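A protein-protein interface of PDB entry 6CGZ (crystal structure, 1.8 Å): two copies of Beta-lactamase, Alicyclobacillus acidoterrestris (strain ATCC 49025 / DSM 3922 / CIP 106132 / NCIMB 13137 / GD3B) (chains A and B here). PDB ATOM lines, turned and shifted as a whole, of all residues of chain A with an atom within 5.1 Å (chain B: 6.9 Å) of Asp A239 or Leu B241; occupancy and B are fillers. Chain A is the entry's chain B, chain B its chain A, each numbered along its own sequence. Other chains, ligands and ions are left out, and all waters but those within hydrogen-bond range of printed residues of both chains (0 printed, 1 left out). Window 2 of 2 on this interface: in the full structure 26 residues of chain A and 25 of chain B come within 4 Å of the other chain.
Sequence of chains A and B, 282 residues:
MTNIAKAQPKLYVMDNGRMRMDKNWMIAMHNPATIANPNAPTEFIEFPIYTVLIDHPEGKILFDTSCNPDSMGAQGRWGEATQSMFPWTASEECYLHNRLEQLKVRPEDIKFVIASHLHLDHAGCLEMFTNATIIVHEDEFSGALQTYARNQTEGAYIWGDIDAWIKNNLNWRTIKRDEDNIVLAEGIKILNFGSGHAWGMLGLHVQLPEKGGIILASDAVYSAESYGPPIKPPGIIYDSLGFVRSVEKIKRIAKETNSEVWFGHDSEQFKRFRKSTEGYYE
The backbone carbonyl oxygen of Ile B237 lies within hydrogen-bond range of the side-chain hydroxyl of Ser A240 (3.2 Å). O of Tyr B238 lies within hydrogen-bond range of OG of Ser A240 (2.7 Å). The side-chain hydroxyl (OG) of Ser B240 sits at hydrogen-bond distance from the backbone carbonyl oxygen (O) of Tyr A238 (2.6 Å). N of Ser A240 lies within hydrogen-bond range of OG of Ser B240, at 2.9 Å.
The backbone NH (N) of Gly B242 sits at hydrogen-bond distance from the side-chain carboxylate (OD1) of Asp B239 (3.0 Å). The side-chain carboxylate (OD2) of Asp A239 is in hydrogen-bond range of the side-chain hydroxyl (OG) of Ser A195 (2.5 Å). The backbone carbonyl oxygen (O) of Gly A196 sits close to the backbone NH (N) of Tyr A238 (3.4 Å). The backbone carbonyl oxygen (O) of Gly A196 lies within hydrogen-bond range of the backbone NH (N) of Asp A239, at 2.9 Å. The side-chain carboxylate (OD1) of Asp A239 lies close to the backbone NH (N) of Leu A241. OD1 of Asp A239 is in hydrogen-bond range of N of Gly A242 (3.0 Å).
Among the printed residues, pairs that only touch across the chains: Asp A239 with Ser B240 (3.3 Å), Ser A240 with Asp B239 (3.3 Å), Tyr A238 with Leu B241 (3.4 Å), Leu A241 with Asp B239 (3.5 Å), Ile A237 with Ser B240 (3.5 Å), Leu A241 with Tyr B238 (3.6 Å) and Asp A239 with Leu B241 (3.6 Å).
Asp A239 touches just these residues of chain B: Ser B240 (3.3 Å) and Leu B241 (3.6 Å). Printed residues of chain A within 4 Å of Tyr B238: Ser A240 (2.7 Å) and Leu A241 (3.6 Å). Of the printed residues of chain A, Asp B239 touches Ser A240 (3.3 Å) and Leu A241 (3.5 Å). Leu B241 touches just these residues of chain A: Tyr A238 and Asp A239. The nearest residue of chain B that does not touch Asp A239 is Asp B239 (5.0 Å). The nearest printed residue of chain B that does not touch Ser A240 is Leu B241 (5.2 Å).
Of the 11 printed residues of chain A, 5 touch a printed residue of chain B. Among the printed residues, 11 pairs touch across the chains. Among the printed residues, no Asp or Glu carboxylate lies within 4 Å of a Lys or Arg side-chain nitrogen of the other chain.
Ile A237 touches Ser B240, and with the chains exchanged Ser A240 touches Ile B237. Tyr A238 touches Leu B241, and with the chains exchanged Leu A241 touches Tyr B238. Asp A239 touches Ser B240, and with the chains exchanged Ser A240 touches Asp B239. Ser B240 touches its own counterpart, Ser A240. Of the 11 pairs that touch across the chains among the printed residues, 11 have their exchanged pair printed and touching as well.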
ATOM      1  N   SER A 195     -10.884  32.263  27.035  1.00  0.00           N
ATOM      2  CA  SER A 195     -10.881  32.334  25.577  1.00  0.00           C
ATOM      3  C   SER A 195     -11.585  31.147  24.920  1.00  0.00           C
ATOM      4  O   SER A 195     -11.541  29.996  25.390  1.00  0.00           O
ATOM      5  CB  SER A 195      -9.456  32.464  25.015  1.00  0.00           C
ATOM      6  OG  SER A 195      -8.692  31.387  25.466  1.00  0.00           O
ATOM      7  N   GLY A 196     -12.276  31.441  23.841  1.00  0.00           N
ATOM      8  CA  GLY A 196     -12.946  30.428  23.060  1.00  0.00           C
ATOM      9  C   GLY A 196     -13.575  31.126  21.883  1.00  0.00           C
ATOM     10  O   GLY A 196     -12.894  31.525  20.910  1.00  0.00           O
ATOM     11  N   HIS A 197     -14.881  31.319  21.974  1.00  0.00           N
ATOM     12  CA  HIS A 197     -15.611  32.107  20.975  1.00  0.00           C
ATOM     13  C   HIS A 197     -14.957  33.448  20.741  1.00  0.00           C
ATOM     14  O   HIS A 197     -14.826  33.882  19.592  1.00  0.00           O
ATOM     15  CB  HIS A 197     -17.064  32.289  21.440  1.00  0.00           C
ATOM     16  CG  HIS A 197     -17.851  33.260  20.631  1.00  0.00           C
ATOM     17  ND1 HIS A 197     -18.376  32.945  19.399  1.00  0.00           N
ATOM     18  CD2 HIS A 197     -18.233  34.537  20.885  1.00  0.00           C
ATOM     19  CE1 HIS A 197     -19.063  33.976  18.942  1.00  0.00           C
ATOM     20  NE2 HIS A 197     -18.975  34.953  19.815  1.00  0.00           N
ATOM     21  N   ILE A 237     -13.693  30.903  14.863  1.00  0.00           N
ATOM     22  CA  ILE A 237     -13.570  30.689  16.280  1.00  0.00           C
ATOM     23  C   ILE A 237     -12.202  31.197  16.678  1.00  0.00           C
ATOM     24  O   ILE A 237     -11.202  30.768  16.080  1.00  0.00           O
ATOM     25  CB  ILE A 237     -13.827  29.190  16.593  1.00  0.00           C
ATOM     26  CG1 ILE A 237     -13.771  28.899  18.090  1.00  0.00           C
ATOM     27  CG2 ILE A 237     -12.876  28.265  15.828  1.00  0.00           C
ATOM     28  CD1 ILE A 237     -14.793  29.692  18.849  1.00  0.00           C
ATOM     29  N   TYR A 238     -12.148  32.102  17.662  1.00  0.00           N
ATOM     30  CA  TYR A 238     -10.869  32.644  18.124  1.00  0.00           C
ATOM     31  C   TYR A 238      -9.942  31.541  18.654  1.00  0.00           C
ATOM     32  O   TYR A 238      -8.830  31.354  18.144  1.00  0.00           O
ATOM     33  CB  TYR A 238     -11.055  33.730  19.199  1.00  0.00           C
ATOM     34  CG  TYR A 238      -9.758  34.133  19.838  1.00  0.00           C
ATOM     35  CD1 TYR A 238      -8.734  34.708  19.076  1.00  0.00           C
ATOM     36  CD2 TYR A 238      -9.505  33.887  21.176  1.00  0.00           C
ATOM     37  CE1 TYR A 238      -7.513  35.036  19.645  1.00  0.00           C
ATOM     38  CE2 TYR A 238      -8.305  34.203  21.739  1.00  0.00           C
ATOM     39  CZ  TYR A 238      -7.323  34.811  20.978  1.00  0.00           C
ATOM     40  OH  TYR A 238      -6.140  35.103  21.558  1.00  0.00           O
ATOM     41  N   ASP A 239     -10.419  30.824  19.673  1.00  0.00           N
ATOM     42  CA  ASP A 239      -9.674  29.763  20.362  1.00  0.00           C
ATOM     43  C   ASP A 239     -10.490  28.439  20.359  1.00  0.00           C
ATOM     44  O   ASP A 239     -11.294  28.179  21.242  1.00  0.00           O
ATOM     45  CB  ASP A 239      -9.312  30.244  21.779  1.00  0.00           C
ATOM     46  CG  ASP A 239      -8.604  29.192  22.632  1.00  0.00           C
ATOM     47  OD1 ASP A 239      -8.222  28.078  22.146  1.00  0.00           O
ATOM     48  OD2 ASP A 239      -8.443  29.486  23.839  1.00  0.00           O
ATOM     49  N   SER A 240     -10.235  27.583  19.370  1.00  0.00           N
ATOM     50  CA  SER A 240     -11.027  26.391  19.192  1.00  0.00           C
ATOM     51  C   SER A 240     -10.877  25.416  20.352  1.00  0.00           C
ATOM     52  O   SER A 240     -11.871  24.793  20.783  1.00  0.00           O
ATOM     53  CB  SER A 240     -10.718  25.761  17.832  1.00  0.00           C
ATOM     54  OG  SER A 240      -9.371  25.344  17.787  1.00  0.00           O
ATOM     55  N   LEU A 241      -9.679  25.288  20.909  1.00  0.00           N
ATOM     56  CA  LEU A 241      -9.506  24.419  22.065  1.00  0.00           C
ATOM     57  C   LEU A 241     -10.237  24.948  23.289  1.00  0.00           C
ATOM     58  O   LEU A 241     -10.834  24.173  24.048  1.00  0.00           O
ATOM     59  CB  LEU A 241      -8.028  24.230  22.388  1.00  0.00           C
ATOM     60  CG  LEU A 241      -7.245  23.392  21.386  1.00  0.00           C
ATOM     61  CD1 LEU A 241      -5.780  23.346  21.823  1.00  0.00           C
ATOM     62  CD2 LEU A 241      -7.842  21.999  21.251  1.00  0.00           C
ATOM     63  N   GLY A 242     -10.147  26.260  23.491  1.00  0.00           N
ATOM     64  CA  GLY A 242     -10.822  26.929  24.605  1.00  0.00           C
ATOM     65  C   GLY A 242     -12.320  26.839  24.446  1.00  0.00           C
ATOM     66  O   GLY A 242     -13.043  26.706  25.424  1.00  0.00           O
ATOM     67  N   PHE A 243     -12.791  26.861  23.208  1.00  0.00           N
ATOM     68  CA  PHE A 243     -14.218  26.703  22.953  1.00  0.00           C
ATOM     69  C   PHE A 243     -14.735  25.358  23.468  1.00  0.00           C
ATOM     70  O   PHE A 243     -15.720  25.290  24.174  1.00  0.00           O
ATOM     71  CB  PHE A 243     -14.559  26.864  21.480  1.00  0.00           C
ATOM     72  CG  PHE A 243     -15.983  26.559  21.189  1.00  0.00           C
ATOM     73  CD1 PHE A 243     -16.964  27.537  21.381  1.00  0.00           C
ATOM     74  CD2 PHE A 243     -16.369  25.297  20.804  1.00  0.00           C
ATOM     75  CE1 PHE A 243     -18.302  27.247  21.148  1.00  0.00           C
ATOM     76  CE2 PHE A 243     -17.722  24.998  20.596  1.00  0.00           C
ATOM     77  CZ  PHE A 243     -18.679  25.979  20.774  1.00  0.00           C
ATOM     78  N   ARG A 245     -13.239  23.269  25.596  1.00  0.00           N
ATOM     79  CA  ARG A 245     -13.024  23.218  27.043  1.00  0.00           C
ATOM     80  C   ARG A 245     -14.157  23.919  27.761  1.00  0.00           C
ATOM     81  O   ARG A 245     -14.684  23.407  28.748  1.00  0.00           O
ATOM     82  CB  ARG A 245     -11.703  23.875  27.442  1.00  0.00           C
ATOM     83  CG  ARG A 245     -10.513  22.925  27.442  1.00  0.00           C
ATOM     84  CD  ARG A 245      -9.280  23.575  28.059  1.00  0.00           C
ATOM     85  NE  ARG A 245      -8.908  24.844  27.438  1.00  0.00           N
ATOM     86  CZ  ARG A 245      -7.950  24.976  26.530  1.00  0.00           C
ATOM     87  NH1 ARG A 245      -7.276  23.919  26.125  1.00  0.00           N
ATOM     88  NH2 ARG A 245      -7.672  26.161  26.031  1.00  0.00           N
ATOM     89  N   SER B 195       0.891  21.790  17.871  1.00  0.00           N
ATOM     90  CA  SER B 195      -0.518  21.635  17.592  1.00  0.00           C
ATOM     91  C   SER B 195      -1.068  22.846  16.820  1.00  0.00           C
ATOM     92  O   SER B 195      -0.644  23.978  17.014  1.00  0.00           O
ATOM     93  CB  SER B 195      -1.298  21.401  18.887  1.00  0.00           C
ATOM     94  OG  SER B 195      -1.426  22.599  19.596  1.00  0.00           O
ATOM     95  N   GLY B 196      -2.031  22.581  15.960  1.00  0.00           N
ATOM     96  CA  GLY B 196      -2.621  23.580  15.088  1.00  0.00           C
ATOM     97  C   GLY B 196      -3.639  22.897  14.215  1.00  0.00           C
ATOM     98  O   GLY B 196      -4.749  22.537  14.660  1.00  0.00           O
ATOM     99  N   ILE B 237     -10.832  23.829  12.405  1.00  0.00           N
ATOM    100  CA  ILE B 237      -9.442  23.832  12.804  1.00  0.00           C
ATOM    101  C   ILE B 237      -9.369  23.251  14.206  1.00  0.00           C
ATOM    102  O   ILE B 237     -10.103  23.711  15.090  1.00  0.00           O
ATOM    103  CB  ILE B 237      -8.826  25.250  12.693  1.00  0.00           C
ATOM    104  CG1 ILE B 237      -7.384  25.239  13.126  1.00  0.00           C
ATOM    105  CG2 ILE B 237      -9.589  26.277  13.535  1.00  0.00           C
ATOM    106  CD1 ILE B 237      -6.485  24.528  12.158  1.00  0.00           C
ATOM    107  N   TYR B 238      -8.499  22.251  14.405  1.00  0.00           N
ATOM    108  CA  TYR B 238      -8.306  21.661  15.727  1.00  0.00           C
ATOM    109  C   TYR B 238      -7.838  22.672  16.795  1.00  0.00           C
ATOM    110  O   TYR B 238      -8.477  22.807  17.832  1.00  0.00           O
ATOM    111  CB  TYR B 238      -7.353  20.464  15.659  1.00  0.00           C
ATOM    112  CG  TYR B 238      -6.913  20.016  17.002  1.00  0.00           C
ATOM    113  CD1 TYR B 238      -7.806  19.391  17.871  1.00  0.00           C
ATOM    114  CD2 TYR B 238      -5.640  20.236  17.438  1.00  0.00           C
ATOM    115  CE1 TYR B 238      -7.414  18.997  19.133  1.00  0.00           C
ATOM    116  CE2 TYR B 238      -5.251  19.874  18.690  1.00  0.00           C
ATOM    117  CZ  TYR B 238      -6.146  19.235  19.534  1.00  0.00           C
ATOM    118  OH  TYR B 238      -5.753  18.876  20.779  1.00  0.00           O
ATOM    119  N   ASP B 239      -6.734  23.372  16.556  1.00  0.00           N
ATOM    120  CA  ASP B 239      -6.194  24.348  17.518  1.00  0.00           C
ATOM    121  C   ASP B 239      -5.940  25.654  16.766  1.00  0.00           C
ATOM    122  O   ASP B 239      -4.873  25.846  16.193  1.00  0.00           O
ATOM    123  CB  ASP B 239      -4.931  23.781  18.182  1.00  0.00           C
ATOM    124  CG  ASP B 239      -4.203  24.774  19.069  1.00  0.00           C
ATOM    125  OD1 ASP B 239      -4.742  25.866  19.387  1.00  0.00           O
ATOM    126  OD2 ASP B 239      -3.045  24.437  19.475  1.00  0.00           O
ATOM    127  N   SER B 240      -6.943  26.540  16.766  1.00  0.00           N
ATOM    128  CA  SER B 240      -6.880  27.787  16.002  1.00  0.00           C
ATOM    129  C   SER B 240      -5.728  28.677  16.454  1.00  0.00           C
ATOM    130  O   SER B 240      -5.043  29.283  15.623  1.00  0.00           O
ATOM    131  CB  SER B 240      -8.233  28.520  16.061  1.00  0.00           C
ATOM    132  OG  SER B 240      -8.547  28.826  17.409  1.00  0.00           O
ATOM    133  N   LEU B 241      -5.469  28.775  17.756  1.00  0.00           N
ATOM    134  CA  LEU B 241      -4.365  29.642  18.221  1.00  0.00           C
ATOM    135  C   LEU B 241      -3.023  29.051  17.759  1.00  0.00           C
ATOM    136  O   LEU B 241      -2.105  29.777  17.358  1.00  0.00           O
ATOM    137  CB  LEU B 241      -4.380  29.793  19.748  1.00  0.00           C
ATOM    138  CG  LEU B 241      -5.616  30.501  20.360  1.00  0.00           C
ATOM    139  CD1 LEU B 241      -5.411  30.601  21.871  1.00  0.00           C
ATOM    140  CD2 LEU B 241      -5.839  31.875  19.749  1.00  0.00           C
ATOM    141  N   GLY B 242      -2.912  27.731  17.864  1.00  0.00           N
ATOM    142  CA  GLY B 242      -1.717  27.022  17.411  1.00  0.00           C
ATOM    143  C   GLY B 242      -1.512  27.186  15.914  1.00  0.00           C
ATOM    144  O   GLY B 242      -0.390  27.334  15.458  1.00  0.00           O
ATOM    145  N   PHE B 243      -2.596  27.152  15.167  1.00  0.00           N
ATOM    146  CA  PHE B 243      -2.543  27.343  13.714  1.00  0.00           C
ATOM    147  C   PHE B 243      -1.886  28.693  13.361  1.00  0.00           C
ATOM    148  O   PHE B 243      -0.918  28.767  12.575  1.00  0.00           O
ATOM    149  CB  PHE B 243      -3.930  27.238  13.106  1.00  0.00           C
ATOM    150  CG  PHE B 243      -3.952  27.627  11.671  1.00  0.00           C
ATOM    151  CD1 PHE B 243      -3.539  26.725  10.712  1.00  0.00           C
ATOM    152  CD2 PHE B 243      -4.297  28.892  11.300  1.00  0.00           C
ATOM    153  CE1 PHE B 243      -3.500  27.093   9.376  1.00  0.00           C
ATOM    154  CE2 PHE B 243      -4.256  29.274   9.958  1.00  0.00           C
ATOM    155  CZ  PHE B 243      -3.851  28.361   9.014  1.00  0.00           C
ATOM    156  N   VAL B 244      -2.374  29.759  14.000  1.00  0.00           N
ATOM    157  CA  VAL B 244      -1.853  31.085  13.733  1.00  0.00           C
ATOM    158  C   VAL B 244      -0.422  31.216  14.189  1.00  0.00           C
ATOM    159  O   VAL B 244       0.395  31.797  13.477  1.00  0.00           O
ATOM    160  CB  VAL B 244      -2.731  32.177  14.407  1.00  0.00           C
ATOM    161  CG1 VAL B 244      -2.064  33.538  14.268  1.00  0.00           C
ATOM    162  CG2 VAL B 244      -4.105  32.158  13.799  1.00  0.00           C
ATOM    163  N   ARG B 245      -0.089  30.696  15.374  1.00  0.00           N
ATOM    164  CA  ARG B 245       1.274  30.754  15.881  1.00  0.00           C
ATOM    165  C   ARG B 245       2.252  30.065  14.910  1.00  0.00           C
ATOM    166  O   ARG B 245       3.366  30.548  14.669  1.00  0.00           O
ATOM    167  CB  ARG B 245       1.338  30.063  17.243  1.00  0.00           C
ATOM    168  CG  ARG B 245       2.704  30.016  17.922  1.00  0.00           C
ATOM    169  CD  ARG B 245       2.812  28.916  18.993  1.00  0.00           C
ATOM    170  NE  ARG B 245       2.631  27.581  18.381  1.00  0.00           N
ATOM    171  CZ  ARG B 245       1.707  26.680  18.716  1.00  0.00           C
ATOM    172  NH1 ARG B 245       1.612  25.513  18.028  1.00  0.00           N
ATOM    173  NH2 ARG B 245       0.887  26.920  19.739  1.00  0.00           N
ATOM    174  N   SER B 246       1.817  28.915  14.396  1.00  0.00           N
ATOM    175  CA  SER B 246       2.604  28.123  13.463  1.00  0.00           C
ATOM    176  C   SER B 246       2.805  28.872  12.120  1.00  0.00           C
ATOM    177  O   SER B 246       3.915  28.862  11.576  1.00  0.00           O
ATOM    178  CB  SER B 246       1.947  26.769  13.242  1.00  0.00           C
ATOM    179  OG  SER B 246       1.870  26.041  14.471  1.00  0.00           O
